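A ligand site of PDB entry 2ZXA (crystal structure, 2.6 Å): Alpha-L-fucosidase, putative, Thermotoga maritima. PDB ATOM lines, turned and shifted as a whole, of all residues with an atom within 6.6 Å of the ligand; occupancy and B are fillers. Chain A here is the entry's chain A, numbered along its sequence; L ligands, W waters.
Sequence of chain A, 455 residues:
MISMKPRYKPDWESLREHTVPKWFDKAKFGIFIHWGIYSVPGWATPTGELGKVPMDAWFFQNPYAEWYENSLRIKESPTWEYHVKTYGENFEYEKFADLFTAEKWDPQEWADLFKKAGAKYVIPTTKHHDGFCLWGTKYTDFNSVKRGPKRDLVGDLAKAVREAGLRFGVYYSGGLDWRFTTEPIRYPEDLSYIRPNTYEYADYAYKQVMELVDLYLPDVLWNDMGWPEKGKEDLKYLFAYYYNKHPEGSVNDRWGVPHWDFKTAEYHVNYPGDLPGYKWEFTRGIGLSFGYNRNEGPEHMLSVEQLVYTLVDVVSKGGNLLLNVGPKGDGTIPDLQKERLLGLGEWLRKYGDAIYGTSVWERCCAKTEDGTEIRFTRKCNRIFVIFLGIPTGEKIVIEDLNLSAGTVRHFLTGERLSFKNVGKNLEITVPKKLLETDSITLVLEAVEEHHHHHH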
ATOM      1  N   PHE A  32      17.544  16.104  10.620  1.00  0.00           N
ATOM      2  CA  PHE A  32      18.056  16.130   9.304  1.00  0.00           C
ATOM      3  C   PHE A  32      16.958  15.401   8.470  1.00  0.00           C
ATOM      4  O   PHE A  32      16.375  14.396   8.940  1.00  0.00           O
ATOM      5  CB  PHE A  32      19.325  15.282   9.301  1.00  0.00           C
ATOM      6  CG  PHE A  32      20.381  15.761   8.364  1.00  0.00           C
ATOM      7  CD1 PHE A  32      20.164  16.907   7.557  1.00  0.00           C
ATOM      8  CD2 PHE A  32      21.656  15.178   8.429  1.00  0.00           C
ATOM      9  CE1 PHE A  32      21.250  17.495   6.821  1.00  0.00           C
ATOM     10  CE2 PHE A  32      22.732  15.725   7.722  1.00  0.00           C
ATOM     11  CZ  PHE A  32      22.556  16.890   6.919  1.00  0.00           C
ATOM     12  N   HIS A  34      16.644  13.692   4.633  1.00  0.00           N
ATOM     13  CA  HIS A  34      17.076  13.393   3.279  1.00  0.00           C
ATOM     14  C   HIS A  34      15.898  12.795   2.539  1.00  0.00           C
ATOM     15  O   HIS A  34      15.558  11.625   2.714  1.00  0.00           O
ATOM     16  CB  HIS A  34      18.254  12.403   3.292  1.00  0.00           C
ATOM     17  CG  HIS A  34      19.553  13.058   3.645  1.00  0.00           C
ATOM     18  ND1 HIS A  34      19.743  13.733   4.831  1.00  0.00           N
ATOM     19  CD2 HIS A  34      20.703  13.183   2.935  1.00  0.00           C
ATOM     20  CE1 HIS A  34      20.963  14.246   4.847  1.00  0.00           C
ATOM     21  NE2 HIS A  34      21.565  13.935   3.717  1.00  0.00           N
ATOM     22  N   LEU A  50      29.377   4.153   8.098  1.00  0.00           N
ATOM     23  CA  LEU A  50      30.472   4.859   7.464  1.00  0.00           C
ATOM     24  C   LEU A  50      31.627   4.905   8.469  1.00  0.00           C
ATOM     25  O   LEU A  50      31.429   5.264   9.639  1.00  0.00           O
ATOM     26  CB  LEU A  50      30.115   6.311   7.110  1.00  0.00           C
ATOM     27  CG  LEU A  50      31.229   7.133   6.407  1.00  0.00           C
ATOM     28  CD1 LEU A  50      31.205   6.727   4.909  1.00  0.00           C
ATOM     29  CD2 LEU A  50      31.045   8.631   6.565  1.00  0.00           C
ATOM     30  N   TYR A  64      24.111   4.042   1.581  1.00  0.00           N
ATOM     31  CA  TYR A  64      23.362   5.287   1.586  1.00  0.00           C
ATOM     32  C   TYR A  64      22.419   5.237   0.411  1.00  0.00           C
ATOM     33  O   TYR A  64      22.827   5.412  -0.743  1.00  0.00           O
ATOM     34  CB  TYR A  64      24.287   6.477   1.435  1.00  0.00           C
ATOM     35  CG  TYR A  64      25.092   6.855   2.655  1.00  0.00           C
ATOM     36  CD1 TYR A  64      24.924   6.196   3.897  1.00  0.00           C
ATOM     37  CD2 TYR A  64      25.987   7.951   2.589  1.00  0.00           C
ATOM     38  CE1 TYR A  64      25.638   6.624   5.058  1.00  0.00           C
ATOM     39  CE2 TYR A  64      26.699   8.397   3.725  1.00  0.00           C
ATOM     40  CZ  TYR A  64      26.527   7.730   4.957  1.00  0.00           C
ATOM     41  OH  TYR A  64      27.244   8.183   6.016  1.00  0.00           O
ATOM     42  N   GLU A  66      20.392   7.368  -0.721  1.00  0.00           N
ATOM     43  CA  GLU A  66      20.276   8.519  -1.571  1.00  0.00           C
ATOM     44  C   GLU A  66      21.410   8.507  -2.632  1.00  0.00           C
ATOM     45  O   GLU A  66      21.483   9.392  -3.465  1.00  0.00           O
ATOM     46  CB  GLU A  66      20.270   9.832  -0.737  1.00  0.00           C
ATOM     47  CG  GLU A  66      21.606  10.198   0.026  1.00  0.00           C
ATOM     48  CD  GLU A  66      21.980   9.223   1.184  1.00  0.00           C
ATOM     49  OE1 GLU A  66      23.025   9.428   1.828  1.00  0.00           O
ATOM     50  OE2 GLU A  66      21.215   8.282   1.461  1.00  0.00           O
ATOM     51  N   TRP A  67      22.293   7.505  -2.613  1.00  0.00           N
ATOM     52  CA  TRP A  67      23.356   7.434  -3.628  1.00  0.00           C
ATOM     53  C   TRP A  67      22.949   6.549  -4.796  1.00  0.00           C
ATOM     54  O   TRP A  67      23.777   6.192  -5.670  1.00  0.00           O
ATOM     55  CB  TRP A  67      24.680   6.917  -3.038  1.00  0.00           C
ATOM     56  CG  TRP A  67      25.526   8.043  -2.420  1.00  0.00           C
ATOM     57  CD1 TRP A  67      25.197   8.836  -1.358  1.00  0.00           C
ATOM     58  CD2 TRP A  67      26.801   8.539  -2.902  1.00  0.00           C
ATOM     59  NE1 TRP A  67      26.145   9.786  -1.156  1.00  0.00           N
ATOM     60  CE2 TRP A  67      27.150   9.626  -2.077  1.00  0.00           C
ATOM     61  CE3 TRP A  67      27.673   8.150  -3.919  1.00  0.00           C
ATOM     62  CZ2 TRP A  67      28.322  10.366  -2.251  1.00  0.00           C
ATOM     63  CZ3 TRP A  67      28.842   8.853  -4.099  1.00  0.00           C
ATOM     64  CH2 TRP A  67      29.160   9.969  -3.245  1.00  0.00           C
ATOM     65  N   THR A 125      17.151  18.400   2.826  1.00  0.00           N
ATOM     66  CA  THR A 125      17.979  18.391   1.654  1.00  0.00           C
ATOM     67  C   THR A 125      17.273  19.241   0.625  1.00  0.00           C
ATOM     68  O   THR A 125      16.193  18.861   0.187  1.00  0.00           O
ATOM     69  CB  THR A 125      18.041  16.964   1.118  1.00  0.00           C
ATOM     70  OG1 THR A 125      16.695  16.434   1.197  1.00  0.00           O
ATOM     71  CG2 THR A 125      19.067  16.054   1.981  1.00  0.00           C
ATOM     72  N   HIS A 128      20.282  17.344  -3.363  1.00  0.00           N
ATOM     73  CA  HIS A 128      21.299  16.403  -3.005  1.00  0.00           C
ATOM     74  C   HIS A 128      22.240  16.128  -4.232  1.00  0.00           C
ATOM     75  O   HIS A 128      22.179  16.800  -5.275  1.00  0.00           O
ATOM     76  CB  HIS A 128      20.641  15.148  -2.473  1.00  0.00           C
ATOM     77  CG  HIS A 128      21.516  14.374  -1.552  1.00  0.00           C
ATOM     78  ND1 HIS A 128      22.313  13.338  -1.997  1.00  0.00           N
ATOM     79  CD2 HIS A 128      21.830  14.565  -0.250  1.00  0.00           C
ATOM     80  CE1 HIS A 128      23.094  12.932  -1.018  1.00  0.00           C
ATOM     81  NE2 HIS A 128      22.821  13.660   0.060  1.00  0.00           N
ATOM     82  N   HIS A 129      23.180  15.209  -4.084  1.00  0.00           N
ATOM     83  CA  HIS A 129      24.077  14.935  -5.182  1.00  0.00           C
ATOM     84  C   HIS A 129      23.433  14.711  -6.582  1.00  0.00           C
ATOM     85  O   HIS A 129      24.087  14.971  -7.621  1.00  0.00           O
ATOM     86  CB  HIS A 129      24.947  13.748  -4.799  1.00  0.00           C
ATOM     87  CG  HIS A 129      25.466  13.825  -3.401  1.00  0.00           C
ATOM     88  ND1 HIS A 129      25.747  15.035  -2.786  1.00  0.00           N
ATOM     89  CD2 HIS A 129      25.877  12.851  -2.558  1.00  0.00           C
ATOM     90  CE1 HIS A 129      26.330  14.794  -1.624  1.00  0.00           C
ATOM     91  NE2 HIS A 129      26.413  13.477  -1.460  1.00  0.00           N
ATOM     92  N   TYR A 171      20.016  22.224   3.652  1.00  0.00           N
ATOM     93  CA  TYR A 171      21.145  21.415   3.246  1.00  0.00           C
ATOM     94  C   TYR A 171      21.354  21.633   1.715  1.00  0.00           C
ATOM     95  O   TYR A 171      20.376  21.657   0.941  1.00  0.00           O
ATOM     96  CB  TYR A 171      20.839  19.968   3.542  1.00  0.00           C
ATOM     97  CG  TYR A 171      21.788  19.043   2.858  1.00  0.00           C
ATOM     98  CD1 TYR A 171      22.730  18.326   3.587  1.00  0.00           C
ATOM     99  CD2 TYR A 171      21.726  18.855   1.439  1.00  0.00           C
ATOM    100  CE1 TYR A 171      23.591  17.424   2.935  1.00  0.00           C
ATOM    101  CE2 TYR A 171      22.564  18.002   0.797  1.00  0.00           C
ATOM    102  CZ  TYR A 171      23.501  17.273   1.540  1.00  0.00           C
ATOM    103  OH  TYR A 171      24.339  16.366   0.933  1.00  0.00           O
ATOM    104  N   LEU A 176      28.811  18.022  -5.076  1.00  0.00           N
ATOM    105  CA  LEU A 176      28.471  17.061  -6.133  1.00  0.00           C
ATOM    106  C   LEU A 176      27.125  17.403  -6.741  1.00  0.00           C
ATOM    107  O   LEU A 176      26.239  17.919  -6.065  1.00  0.00           O
ATOM    108  CB  LEU A 176      28.390  15.627  -5.569  1.00  0.00           C
ATOM    109  CG  LEU A 176      29.581  14.974  -4.858  1.00  0.00           C
ATOM    110  CD1 LEU A 176      29.144  13.555  -4.313  1.00  0.00           C
ATOM    111  CD2 LEU A 176      30.840  14.887  -5.786  1.00  0.00           C
ATOM    112  N   TRP A 222      23.918  24.457   5.511  1.00  0.00           N
ATOM    113  CA  TRP A 222      24.652  23.192   5.739  1.00  0.00           C
ATOM    114  C   TRP A 222      25.103  22.652   4.392  1.00  0.00           C
ATOM    115  O   TRP A 222      24.350  21.924   3.745  1.00  0.00           O
ATOM    116  CB  TRP A 222      23.735  22.163   6.404  1.00  0.00           C
ATOM    117  CG  TRP A 222      24.369  21.180   7.323  1.00  0.00           C
ATOM    118  CD1 TRP A 222      24.392  21.241   8.720  1.00  0.00           C
ATOM    119  CD2 TRP A 222      25.033  19.949   6.970  1.00  0.00           C
ATOM    120  NE1 TRP A 222      25.037  20.118   9.237  1.00  0.00           N
ATOM    121  CE2 TRP A 222      25.431  19.311   8.186  1.00  0.00           C
ATOM    122  CE3 TRP A 222      25.325  19.316   5.761  1.00  0.00           C
ATOM    123  CZ2 TRP A 222      26.084  18.074   8.211  1.00  0.00           C
ATOM    124  CZ3 TRP A 222      25.978  18.114   5.776  1.00  0.00           C
ATOM    125  CH2 TRP A 222      26.347  17.491   7.023  1.00  0.00           C
ATOM    126  N   ASP A 224      27.411  20.344   1.754  1.00  0.00           N
ATOM    127  CA  ASP A 224      28.031  19.035   1.797  1.00  0.00           C
ATOM    128  C   ASP A 224      29.022  18.890   0.613  1.00  0.00           C
ATOM    129  O   ASP A 224      28.878  19.510  -0.454  1.00  0.00           O
ATOM    130  CB  ASP A 224      26.966  17.936   1.710  1.00  0.00           C
ATOM    131  CG  ASP A 224      27.407  16.635   2.411  1.00  0.00           C
ATOM    132  OD1 ASP A 224      26.620  15.665   2.494  1.00  0.00           O
ATOM    133  OD2 ASP A 224      28.529  16.583   2.910  1.00  0.00           O
ATOM    134  N   MET A 225      30.069  18.143   0.880  1.00  0.00           N
ATOM    135  CA  MET A 225      31.026  17.714  -0.115  1.00  0.00           C
ATOM    136  C   MET A 225      31.910  18.747  -0.717  1.00  0.00           C
ATOM    137  O   MET A 225      32.420  18.567  -1.815  1.00  0.00           O
ATOM    138  CB  MET A 225      30.267  16.917  -1.216  1.00  0.00           C
ATOM    139  CG  MET A 225      29.689  15.548  -0.763  1.00  0.00           C
ATOM    140  SD  MET A 225      31.004  14.208  -0.388  1.00  0.00           S
ATOM    141  CE  MET A 225      32.059  14.352  -1.802  1.00  0.00           C
ATOM    142  N   ARG A 254      31.748  22.211   5.831  1.00  0.00           N
ATOM    143  CA  ARG A 254      32.045  21.413   4.681  1.00  0.00           C
ATOM    144  C   ARG A 254      32.206  22.186   3.373  1.00  0.00           C
ATOM    145  O   ARG A 254      31.873  21.682   2.310  1.00  0.00           O
ATOM    146  CB  ARG A 254      30.967  20.334   4.523  1.00  0.00           C
ATOM    147  CG  ARG A 254      30.792  19.481   5.747  1.00  0.00           C
ATOM    148  CD  ARG A 254      29.934  18.313   5.429  1.00  0.00           C
ATOM    149  NE  ARG A 254      30.046  17.378   6.512  1.00  0.00           N
ATOM    150  CZ  ARG A 254      29.612  16.128   6.475  1.00  0.00           C
ATOM    151  NH1 ARG A 254      29.764  15.346   7.547  1.00  0.00           N
ATOM    152  NH2 ARG A 254      29.042  15.658   5.398  1.00  0.00           N
ATOM    153  N   GLU A 266      30.376  12.429  10.979  1.00  0.00           N
ATOM    154  CA  GLU A 266      29.381  11.571  10.333  1.00  0.00           C
ATOM    155  C   GLU A 266      29.712  10.056  10.644  1.00  0.00           C
ATOM    156  O   GLU A 266      30.795   9.561  10.350  1.00  0.00           O
ATOM    157  CB  GLU A 266      29.357  11.953   8.855  1.00  0.00           C
ATOM    158  CG  GLU A 266      28.455  11.134   7.952  1.00  0.00           C
ATOM    159  CD  GLU A 266      28.308  11.735   6.565  1.00  0.00           C
ATOM    160  OE1 GLU A 266      28.072  10.953   5.632  1.00  0.00           O
ATOM    161  OE2 GLU A 266      28.425  12.978   6.406  1.00  0.00           O
ATOM    162  N   VAL A 269      33.270   8.777  11.202  1.00  0.00           N
ATOM    163  CA  VAL A 269      34.092   9.821  10.630  1.00  0.00           C
ATOM    164  C   VAL A 269      34.142  11.112  11.407  1.00  0.00           C
ATOM    165  O   VAL A 269      33.112  11.796  11.544  1.00  0.00           O
ATOM    166  CB  VAL A 269      33.656  10.074   9.176  1.00  0.00           C
ATOM    167  CG1 VAL A 269      34.470  11.231   8.523  1.00  0.00           C
ATOM    168  CG2 VAL A 269      33.845   8.791   8.396  1.00  0.00           C
ATOM    169  N   ASN A 270      35.333  11.412  11.939  1.00  0.00           N
ATOM    170  CA  ASN A 270      35.607  12.626  12.741  1.00  0.00           C
ATOM    171  C   ASN A 270      34.977  12.733  14.139  1.00  0.00           C
ATOM    172  O   ASN A 270      34.790  13.828  14.683  1.00  0.00           O
ATOM    173  CB  ASN A 270      35.225  13.886  11.938  1.00  0.00           C
ATOM    174  CG  ASN A 270      36.128  14.118  10.751  1.00  0.00           C
ATOM    175  OD1 ASN A 270      37.346  13.874  10.831  1.00  0.00           O
ATOM    176  ND2 ASN A 270      35.564  14.587   9.641  1.00  0.00           N
ATOM    177  N   THR A 283      26.224  13.716  12.969  1.00  0.00           N
ATOM    178  CA  THR A 283      25.069  13.395  12.131  1.00  0.00           C
ATOM    179  C   THR A 283      25.107  11.914  11.721  1.00  0.00           C
ATOM    180  O   THR A 283      26.178  11.319  11.569  1.00  0.00           O
ATOM    181  CB  THR A 283      25.044  14.327  10.877  1.00  0.00           C
ATOM    182  OG1 THR A 283      23.749  14.342  10.306  1.00  0.00           O
ATOM    183  CG2 THR A 283      26.025  13.864   9.801  1.00  0.00           C
ATOM    184  N   PHE A 290      20.719   7.721   4.776  1.00  0.00           N
ATOM    185  CA  PHE A 290      20.066   9.000   5.093  1.00  0.00           C
ATOM    186  C   PHE A 290      18.722   8.978   4.339  1.00  0.00           C
ATOM    187  O   PHE A 290      17.687   9.341   4.841  1.00  0.00           O
ATOM    188  CB  PHE A 290      20.931  10.203   4.702  1.00  0.00           C
ATOM    189  CG  PHE A 290      22.044  10.451   5.643  1.00  0.00           C
ATOM    190  CD1 PHE A 290      23.242   9.702   5.550  1.00  0.00           C
ATOM    191  CD2 PHE A 290      21.903  11.396   6.691  1.00  0.00           C
ATOM    192  CE1 PHE A 290      24.283   9.911   6.511  1.00  0.00           C
ATOM    193  CE2 PHE A 290      22.920  11.607   7.631  1.00  0.00           C
ATOM    194  CZ  PHE A 290      24.107  10.880   7.555  1.00  0.00           C
HETATM  195  C1  LIG L   1      31.665  12.586   5.257  1.00  0.00           C
HETATM  196  C2  LIG L   1      30.965  13.047   3.973  1.00  0.00           C
HETATM  197  O1  LIG L   1      31.572  13.718   3.151  1.00  0.00           O
HETATM  198  N1  LIG L   1      29.681  12.696   3.859  1.00  0.00           N
HETATM  199  C3  LIG L   1      28.849  13.058   2.704  1.00  0.00           C
HETATM  200  C4  LIG L   1      27.430  12.541   2.967  1.00  0.00           C
HETATM  201  N2  LIG L   1      26.720  13.410   3.931  1.00  0.00           N
HETATM  202  C5  LIG L   1      25.475  12.754   4.356  1.00  0.00           C
HETATM  203  C6  LIG L   1      24.721  13.623   5.361  1.00  0.00           C
HETATM  204  C7  LIG L   1      24.553  12.420   3.177  1.00  0.00           C
HETATM  205  O2  LIG L   1      23.958  13.601   2.634  1.00  0.00           O
HETATM  206  C8  LIG L   1      25.315  11.684   2.074  1.00  0.00           C
HETATM  207  O3  LIG L   1      24.482  11.547   0.930  1.00  0.00           O
HETATM  208  C9  LIG L   1      26.551  12.509   1.706  1.00  0.00           C
HETATM  209  O4  LIG L   1      27.214  11.858   0.618  1.00  0.00           O
HETATM  210  O   HOH W   1      32.209  16.301   3.060  1.00  0.00           O
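OE2 of Glu 266 is in salt-bridge range of N2 of the ligand (3.0 Å). An oxygen (O2) of the ligand sits at hydrogen-bond distance from the side-chain hydroxyl of Tyr 171 (3.3 Å). NE1 of Trp 67 lies within hydrogen-bond range of O4 of the ligand, at 2.9 Å. The side-chain carboxylate (OE1) of Glu 66 sits at hydrogen-bond distance from an oxygen (O3) of the ligand (2.7 Å). An oxygen (O2) of the ligand is in hydrogen-bond range of a ring nitrogen (NE2) of His 128 (2.8 Å). An oxygen (O4) of the ligand is in hydrogen-bond range of a ring nitrogen (NE2) of His 129 (2.8 Å). A ring nitrogen (NE2) of His 34 sits at hydrogen-bond distance from an oxygen (O2) of the ligand (2.6 Å). A nitrogen (N2) of the ligand is in salt-bridge range of the side-chain carboxylate (OD1) of Asp 224, at 2.7 Å.
OE2 of Glu 266 is in salt-bridge range of NH2 of Arg 254. The side-chain carboxylate of Glu 266 is in hydrogen-bond range of the side-chain hydroxyl of Tyr 64, at 2.9 Å. OH of Tyr 171 lies within hydrogen-bond range of OD1 of Asp 224, 2.9 Å away. OE2 of Glu 66 sits at hydrogen-bond distance from N of Phe 290 (3.4 Å). The side-chain carboxylate of Asp 224 is in salt-bridge range of the guanidinium group of Arg 254. The side-chain hydroxyl (OH) of Tyr 171 is in hydrogen-bond range of a ring nitrogen (NE2) of His 128 (3.2 Å).
SD of Met 225 lies close to O1 of the ligand (3.6 Å). The guanidinium group (NH2) of Arg 254 lies close to a nitrogen (N1) of the ligand, 3.4 Å away. CE2 of Phe 32 touches C6 of the ligand (3.7 Å). CD2 of Tyr 64 touches C8 of the ligand, at 3.8 Å. Phe 290 touches the ligand (CE2 to C6, 3.5 Å). Hydrophobic or aromatic side chains within 4 Å of the ligand: Phe 32, His 34, Tyr 64, Trp 67, His 128, His 129, Tyr 171, Met 225 and Phe 290. Within 4 Å of the ligand: Phe 32, His 34, Tyr 64, Glu 66, Trp 67, His 128, His 129, Tyr 171, Asp 224, Met 225, Arg 254, Glu 266 and Phe 290. Along chain A the residues within 4 Å of the ligand span positions 32 to 290.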
